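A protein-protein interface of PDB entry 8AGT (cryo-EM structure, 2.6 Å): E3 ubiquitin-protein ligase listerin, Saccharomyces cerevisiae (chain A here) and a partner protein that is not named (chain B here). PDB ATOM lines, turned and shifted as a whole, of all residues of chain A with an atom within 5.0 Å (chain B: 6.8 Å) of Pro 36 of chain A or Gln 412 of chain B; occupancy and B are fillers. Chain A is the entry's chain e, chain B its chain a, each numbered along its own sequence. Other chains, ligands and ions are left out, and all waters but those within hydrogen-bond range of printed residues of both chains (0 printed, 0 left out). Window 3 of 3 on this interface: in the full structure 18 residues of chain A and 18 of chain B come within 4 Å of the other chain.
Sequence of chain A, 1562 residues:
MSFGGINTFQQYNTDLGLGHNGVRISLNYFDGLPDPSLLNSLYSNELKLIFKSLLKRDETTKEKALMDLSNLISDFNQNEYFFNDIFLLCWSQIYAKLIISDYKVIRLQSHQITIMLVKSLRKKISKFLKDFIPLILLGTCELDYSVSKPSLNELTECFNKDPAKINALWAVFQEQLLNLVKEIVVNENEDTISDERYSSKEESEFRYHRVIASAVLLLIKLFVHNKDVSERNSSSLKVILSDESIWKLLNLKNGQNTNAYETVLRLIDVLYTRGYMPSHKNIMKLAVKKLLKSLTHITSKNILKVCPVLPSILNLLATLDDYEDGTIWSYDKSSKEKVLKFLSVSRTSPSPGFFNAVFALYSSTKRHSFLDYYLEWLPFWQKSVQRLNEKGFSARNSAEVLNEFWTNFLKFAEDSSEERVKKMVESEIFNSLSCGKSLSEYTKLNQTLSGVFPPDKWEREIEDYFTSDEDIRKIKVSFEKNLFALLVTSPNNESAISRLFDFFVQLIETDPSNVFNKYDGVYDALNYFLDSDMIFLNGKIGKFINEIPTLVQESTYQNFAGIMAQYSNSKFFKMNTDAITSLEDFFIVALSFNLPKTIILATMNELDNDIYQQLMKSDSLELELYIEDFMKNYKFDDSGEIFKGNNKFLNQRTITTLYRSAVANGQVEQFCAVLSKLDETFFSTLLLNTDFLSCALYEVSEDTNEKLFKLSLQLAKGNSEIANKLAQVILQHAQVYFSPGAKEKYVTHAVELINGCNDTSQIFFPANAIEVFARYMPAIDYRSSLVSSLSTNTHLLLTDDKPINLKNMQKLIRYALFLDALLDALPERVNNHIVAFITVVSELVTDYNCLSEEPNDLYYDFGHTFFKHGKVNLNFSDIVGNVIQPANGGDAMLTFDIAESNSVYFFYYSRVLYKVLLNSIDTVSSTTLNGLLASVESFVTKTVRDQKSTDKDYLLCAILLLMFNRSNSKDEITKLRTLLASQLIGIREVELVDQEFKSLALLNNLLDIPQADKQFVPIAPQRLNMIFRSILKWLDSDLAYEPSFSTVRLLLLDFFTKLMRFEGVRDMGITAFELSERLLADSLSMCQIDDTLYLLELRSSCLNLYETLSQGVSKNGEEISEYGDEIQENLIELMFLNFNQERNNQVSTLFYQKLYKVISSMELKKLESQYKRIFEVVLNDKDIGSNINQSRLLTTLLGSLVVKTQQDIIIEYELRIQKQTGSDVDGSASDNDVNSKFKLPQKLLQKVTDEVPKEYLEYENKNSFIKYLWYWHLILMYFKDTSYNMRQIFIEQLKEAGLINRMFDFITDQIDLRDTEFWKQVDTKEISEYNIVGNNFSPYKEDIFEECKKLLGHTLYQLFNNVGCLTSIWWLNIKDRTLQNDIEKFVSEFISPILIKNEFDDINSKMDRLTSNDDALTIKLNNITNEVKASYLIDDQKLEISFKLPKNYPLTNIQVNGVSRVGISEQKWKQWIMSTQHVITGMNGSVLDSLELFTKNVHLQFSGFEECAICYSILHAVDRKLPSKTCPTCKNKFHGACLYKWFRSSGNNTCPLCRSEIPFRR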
ATOM      1  N   PHE A   3      13.241  15.563  14.856  1.00  0.00           N
ATOM      2  CA  PHE A   3      13.483  14.144  14.632  1.00  0.00           C
ATOM      3  C   PHE A   3      14.972  13.927  14.433  1.00  0.00           C
ATOM      4  O   PHE A   3      15.608  14.658  13.678  1.00  0.00           O
ATOM      5  CB  PHE A   3      12.704  13.637  13.421  1.00  0.00           C
ATOM      6  CG  PHE A   3      11.217  13.785  13.547  1.00  0.00           C
ATOM      7  CD1 PHE A   3      10.472  12.843  14.231  1.00  0.00           C
ATOM      8  CD2 PHE A   3      10.561  14.859  12.972  1.00  0.00           C
ATOM      9  CE1 PHE A   3       9.101  12.971  14.343  1.00  0.00           C
ATOM     10  CE2 PHE A   3       9.192  14.995  13.081  1.00  0.00           C
ATOM     11  CZ  PHE A   3       8.460  14.048  13.766  1.00  0.00           C
ATOM     12  N   GLY A   4      15.537  12.935  15.110  1.00  0.00           N
ATOM     13  CA  GLY A   4      16.969  12.709  15.026  1.00  0.00           C
ATOM     14  C   GLY A   4      17.354  11.278  14.728  1.00  0.00           C
ATOM     15  O   GLY A   4      16.577  10.362  14.988  1.00  0.00           O
ATOM     16  N   GLY A   5      18.545  11.076  14.179  1.00  0.00           N
ATOM     17  CA  GLY A   5      19.016   9.737  13.875  1.00  0.00           C
ATOM     18  C   GLY A   5      18.912   9.331  12.424  1.00  0.00           C
ATOM     19  O   GLY A   5      18.151   9.924  11.662  1.00  0.00           O
ATOM     20  N   ILE A   6      19.688   8.328  12.026  1.00  0.00           N
ATOM     21  CA  ILE A   6      19.687   7.869  10.640  1.00  0.00           C
ATOM     22  C   ILE A   6      19.470   6.367  10.614  1.00  0.00           C
ATOM     23  O   ILE A   6      20.007   5.655  11.461  1.00  0.00           O
ATOM     24  CB  ILE A   6      21.037   8.188   9.959  1.00  0.00           C
ATOM     25  CG1 ILE A   6      21.250   9.699   9.859  1.00  0.00           C
ATOM     26  CG2 ILE A   6      21.118   7.588   8.564  1.00  0.00           C
ATOM     27  CD1 ILE A   6      20.292  10.384   8.908  1.00  0.00           C
ATOM     28  N   ASN A   7      18.685   5.871   9.663  1.00  0.00           N
ATOM     29  CA  ASN A   7      18.516   4.431   9.534  1.00  0.00           C
ATOM     30  C   ASN A   7      19.684   3.914   8.725  1.00  0.00           C
ATOM     31  O   ASN A   7      19.519   3.514   7.575  1.00  0.00           O
ATOM     32  CB  ASN A   7      17.207   4.107   8.823  1.00  0.00           C
ATOM     33  CG  ASN A   7      16.001   4.243   9.729  1.00  0.00           C
ATOM     34  OD1 ASN A   7      16.095   4.049  10.940  1.00  0.00           O
ATOM     35  ND2 ASN A   7      14.852   4.563   9.144  1.00  0.00           N
ATOM     36  N   PRO A  34       9.226   5.116   9.792  1.00  0.00           N
ATOM     37  CA  PRO A  34       9.561   6.248   8.921  1.00  0.00           C
ATOM     38  C   PRO A  34      10.895   6.887   9.277  1.00  0.00           C
ATOM     39  O   PRO A  34      11.199   7.055  10.456  1.00  0.00           O
ATOM     40  CB  PRO A  34       8.421   7.231   9.179  1.00  0.00           C
ATOM     41  CG  PRO A  34       7.287   6.386   9.648  1.00  0.00           C
ATOM     42  CD  PRO A  34       7.915   5.280  10.440  1.00  0.00           C
ATOM     43  N   ASP A  35      11.681   7.241   8.267  1.00  0.00           N
ATOM     44  CA  ASP A  35      12.994   7.834   8.501  1.00  0.00           C
ATOM     45  C   ASP A  35      12.871   9.198   9.153  1.00  0.00           C
ATOM     46  O   ASP A  35      11.994   9.979   8.797  1.00  0.00           O
ATOM     47  CB  ASP A  35      13.744   7.967   7.177  1.00  0.00           C
ATOM     48  CG  ASP A  35      15.238   8.131   7.365  1.00  0.00           C
ATOM     49  OD1 ASP A  35      15.882   7.190   7.874  1.00  0.00           O
ATOM     50  OD2 ASP A  35      15.769   9.195   6.997  1.00  0.00           O
ATOM     51  N   PRO A  36      13.764   9.499  10.102  1.00  0.00           N
ATOM     52  CA  PRO A  36      13.672  10.773  10.815  1.00  0.00           C
ATOM     53  C   PRO A  36      13.824  11.989   9.913  1.00  0.00           C
ATOM     54  O   PRO A  36      13.113  12.969  10.098  1.00  0.00           O
ATOM     55  CB  PRO A  36      14.839  10.697  11.789  1.00  0.00           C
ATOM     56  CG  PRO A  36      14.948   9.242  12.090  1.00  0.00           C
ATOM     57  CD  PRO A  36      14.677   8.562  10.779  1.00  0.00           C
ATOM     58  N   SER A  37      14.736  11.931   8.953  1.00  0.00           N
ATOM     59  CA  SER A  37      14.926  13.051   8.047  1.00  0.00           C
ATOM     60  C   SER A  37      13.671  13.306   7.228  1.00  0.00           C
ATOM     61  O   SER A  37      13.288  14.452   7.016  1.00  0.00           O
ATOM     62  CB  SER A  37      16.112  12.802   7.121  1.00  0.00           C
ATOM     63  OG  SER A  37      15.827  11.774   6.190  1.00  0.00           O
ATOM     64  N   LEU A  38      13.028  12.243   6.764  1.00  0.00           N
ATOM     65  CA  LEU A  38      11.797  12.392   5.999  1.00  0.00           C
ATOM     66  C   LEU A  38      10.718  13.013   6.871  1.00  0.00           C
ATOM     67  O   LEU A  38       9.948  13.857   6.415  1.00  0.00           O
ATOM     68  CB  LEU A  38      11.339  11.036   5.465  1.00  0.00           C
ATOM     69  CG  LEU A  38      10.612  11.010   4.119  1.00  0.00           C
ATOM     70  CD1 LEU A  38      11.465  11.646   3.034  1.00  0.00           C
ATOM     71  CD2 LEU A  38      10.242   9.583   3.743  1.00  0.00           C
ATOM     72  N   LEU A  39      10.655  12.596   8.128  1.00  0.00           N
ATOM     73  CA  LEU A  39       9.678  13.158   9.049  1.00  0.00           C
ATOM     74  C   LEU A  39       9.943  14.641   9.237  1.00  0.00           C
ATOM     75  O   LEU A  39       9.006  15.433   9.307  1.00  0.00           O
ATOM     76  CB  LEU A  39       9.724  12.421  10.382  1.00  0.00           C
ATOM     77  CG  LEU A  39       9.178  10.996  10.372  1.00  0.00           C
ATOM     78  CD1 LEU A  39       9.558  10.247  11.640  1.00  0.00           C
ATOM     79  CD2 LEU A  39       7.671  11.018  10.183  1.00  0.00           C
ATOM     80  N   ASN A  40      11.213  15.025   9.317  1.00  0.00           N
ATOM     81  CA  ASN A  40      11.570  16.436   9.435  1.00  0.00           C
ATOM     82  C   ASN A  40      11.113  17.184   8.200  1.00  0.00           C
ATOM     83  O   ASN A  40      10.679  18.329   8.289  1.00  0.00           O
ATOM     84  CB  ASN A  40      13.079  16.597   9.585  1.00  0.00           C
ATOM     85  CG  ASN A  40      13.567  16.268  10.977  1.00  0.00           C
ATOM     86  OD1 ASN A  40      13.010  16.735  11.969  1.00  0.00           O
ATOM     87  ND2 ASN A  40      14.629  15.477  11.058  1.00  0.00           N
ATOM     88  N   GLN B 407      24.758   4.142  16.932  1.00  0.00           N
ATOM     89  CA  GLN B 407      24.455   5.421  17.541  1.00  0.00           C
ATOM     90  C   GLN B 407      23.241   6.033  16.888  1.00  0.00           C
ATOM     91  O   GLN B 407      22.417   6.629  17.560  1.00  0.00           O
ATOM     92  CB  GLN B 407      25.646   6.367  17.447  1.00  0.00           C
ATOM     93  CG  GLN B 407      25.533   7.586  18.345  1.00  0.00           C
ATOM     94  CD  GLN B 407      25.455   7.219  19.812  1.00  0.00           C
ATOM     95  OE1 GLN B 407      24.603   7.722  20.544  1.00  0.00           O
ATOM     96  NE2 GLN B 407      26.341   6.331  20.250  1.00  0.00           N
ATOM     97  N   GLY B 408      23.120   5.882  15.579  1.00  0.00           N
ATOM     98  CA  GLY B 408      22.011   6.492  14.881  1.00  0.00           C
ATOM     99  C   GLY B 408      20.701   5.948  15.395  1.00  0.00           C
ATOM    100  O   GLY B 408      19.747   6.700  15.586  1.00  0.00           O
ATOM    101  N   LEU B 409      20.639   4.645  15.632  1.00  0.00           N
ATOM    102  CA  LEU B 409      19.430   4.066  16.196  1.00  0.00           C
ATOM    103  C   LEU B 409      19.155   4.599  17.597  1.00  0.00           C
ATOM    104  O   LEU B 409      18.012   4.899  17.935  1.00  0.00           O
ATOM    105  CB  LEU B 409      19.533   2.546  16.208  1.00  0.00           C
ATOM    106  CG  LEU B 409      19.716   1.902  14.834  1.00  0.00           C
ATOM    107  CD1 LEU B 409      18.462   2.082  13.995  1.00  0.00           C
ATOM    108  CD2 LEU B 409      20.924   2.492  14.124  1.00  0.00           C
ATOM    109  N   ILE B 410      20.196   4.722  18.414  1.00  0.00           N
ATOM    110  CA  ILE B 410      20.035   5.255  19.767  1.00  0.00           C
ATOM    111  C   ILE B 410      19.567   6.696  19.715  1.00  0.00           C
ATOM    112  O   ILE B 410      18.713   7.106  20.497  1.00  0.00           O
ATOM    113  CB  ILE B 410      21.341   5.151  20.572  1.00  0.00           C
ATOM    114  CG1 ILE B 410      21.791   3.696  20.655  1.00  0.00           C
ATOM    115  CG2 ILE B 410      21.169   5.706  21.975  1.00  0.00           C
ATOM    116  CD1 ILE B 410      23.029   3.502  21.495  1.00  0.00           C
ATOM    117  N   ASP B 411      20.099   7.464  18.775  1.00  0.00           N
ATOM    118  CA  ASP B 411      19.707   8.858  18.626  1.00  0.00           C
ATOM    119  C   ASP B 411      18.235   8.937  18.298  1.00  0.00           C
ATOM    120  O   ASP B 411      17.545   9.849  18.740  1.00  0.00           O
ATOM    121  CB  ASP B 411      20.532   9.534  17.542  1.00  0.00           C
ATOM    122  CG  ASP B 411      21.987   9.677  17.927  1.00  0.00           C
ATOM    123  OD1 ASP B 411      22.306   9.502  19.122  1.00  0.00           O
ATOM    124  OD2 ASP B 411      22.814   9.961  17.036  1.00  0.00           O
ATOM    125  N   GLN B 412      17.749   7.983  17.519  1.00  0.00           N
ATOM    126  CA  GLN B 412      16.336   7.945  17.185  1.00  0.00           C
ATOM    127  C   GLN B 412      15.492   7.782  18.437  1.00  0.00           C
ATOM    128  O   GLN B 412      14.357   8.248  18.483  1.00  0.00           O
ATOM    129  CB  GLN B 412      16.047   6.819  16.205  1.00  0.00           C
ATOM    130  CG  GLN B 412      16.905   6.876  14.960  1.00  0.00           C
ATOM    131  CD  GLN B 412      16.327   6.060  13.828  1.00  0.00           C
ATOM    132  OE1 GLN B 412      15.292   5.413  13.977  1.00  0.00           O
ATOM    133  NE2 GLN B 412      16.988   6.095  12.686  1.00  0.00           N
ATOM    134  N   GLN B 413      16.034   7.121  19.451  1.00  0.00           N
ATOM    135  CA  GLN B 413      15.273   6.889  20.668  1.00  0.00           C
ATOM    136  C   GLN B 413      14.383   5.672  20.570  1.00  0.00           C
ATOM    137  O   GLN B 413      13.412   5.546  21.311  1.00  0.00           O
ATOM    138  CB  GLN B 413      14.450   8.121  21.020  1.00  0.00           C
ATOM    139  CG  GLN B 413      15.235   9.204  21.738  1.00  0.00           C
ATOM    140  CD  GLN B 413      14.348  10.324  22.237  1.00  0.00           C
ATOM    141  OE1 GLN B 413      14.814  11.253  22.894  1.00  0.00           O
ATOM    142  NE2 GLN B 413      13.060  10.240  21.927  1.00  0.00           N
ATOM    143  N   MET B 414      14.694   4.781  19.642  1.00  0.00           N
ATOM    144  CA  MET B 414      13.931   3.549  19.509  1.00  0.00           C
ATOM    145  C   MET B 414      14.151   2.674  20.733  1.00  0.00           C
ATOM    146  O   MET B 414      15.198   2.752  21.371  1.00  0.00           O
ATOM    147  CB  MET B 414      14.371   2.805  18.251  1.00  0.00           C
ATOM    148  CG  MET B 414      13.349   1.821  17.711  1.00  0.00           C
ATOM    149  SD  MET B 414      13.994   0.833  16.347  1.00  0.00           S
ATOM    150  CE  MET B 414      14.411   2.114  15.168  1.00  0.00           C
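O of Gly 4 of chain A touches O of Asp 411 of chain B, 3.9 Å away. CA of Gln 412 of chain B touches O of Gly 4 of chain A (3.3 Å). O of Gly 408 of chain B touches CA of Gly 5 of chain A, at 3.6 Å. CA of Gly 5 of chain A touches CB of Asp 411 of chain B, at 3.97 Å. Gly 5 of chain A touches Gln 412 of chain B (CA to CG, 3.7 Å). N of Ile 6 of chain A touches O of Gly 408 of chain B, 3.9 Å away. Pro 36 of chain A touches Gln 412 of chain B (CG to NE2, 3.8 Å).
The side-chain amide oxygen (OE1) of Gln 407 of chain B lies close to the side-chain carboxylate (OD1) of Asp 411 of chain B. The side-chain amide nitrogen (ND2) of Asn 40 of chain A is in hydrogen-bond range of the backbone carbonyl oxygen (O) of Pro 36 of chain A (3.1 Å). The side-chain carboxylate of Asp 35 of chain A sits at hydrogen-bond distance from the side-chain amide nitrogen of Asn 7 of chain A, at 3.1 Å.
Of the printed residues of chain B, Pro 36 of chain A touches Gln 412. Of chain A, only Gly 4 (3.3 Å), Gly 5 (3.7 Å), Ile 6 (3.2 Å), Asn 7 (2.8 Å) and Pro 36 (3.8 Å) come within 4 Å of Gln 412 of chain B. Printed residues of chain A within 4 Å of Asp 411 of chain B: Gly 4 (3.9 Å) and Gly 5 (3.97 Å). Of the printed residues of chain B, Gly 4 of chain A touches Asp 411 (3.9 Å) and Gln 412 (3.3 Å). Of the printed residues of chain B, Ile 6 of chain A touches Gly 408 (3.9 Å) and Gln 412 (3.2 Å). Printed residues of chain B within 4 Å of Gly 5 of chain A: Gly 408, Asp 411 and Gln 412. Leu 38 of chain A touches none of the printed residues of chain B. The nearest residue of chain B that does not touch Pro 36 of chain A is Gly 408 of chain B (6.5 Å). The nearest printed residue of chain A that does not touch Gln 412 of chain B is Asp 35 of chain A (5.1 Å). The nearest printed residue of chain B that does not touch Gly 4 of chain A is Gly 408 of chain B (4.9 Å).
O of Ile 6 of chain A sits close to NE2 of Gln 412 of chain B (3.3 Å). The side-chain amide oxygen (OD1) of Asn 7 of chain A sits at hydrogen-bond distance from the side-chain amide nitrogen (NE2) of Gln 412 of chain B.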
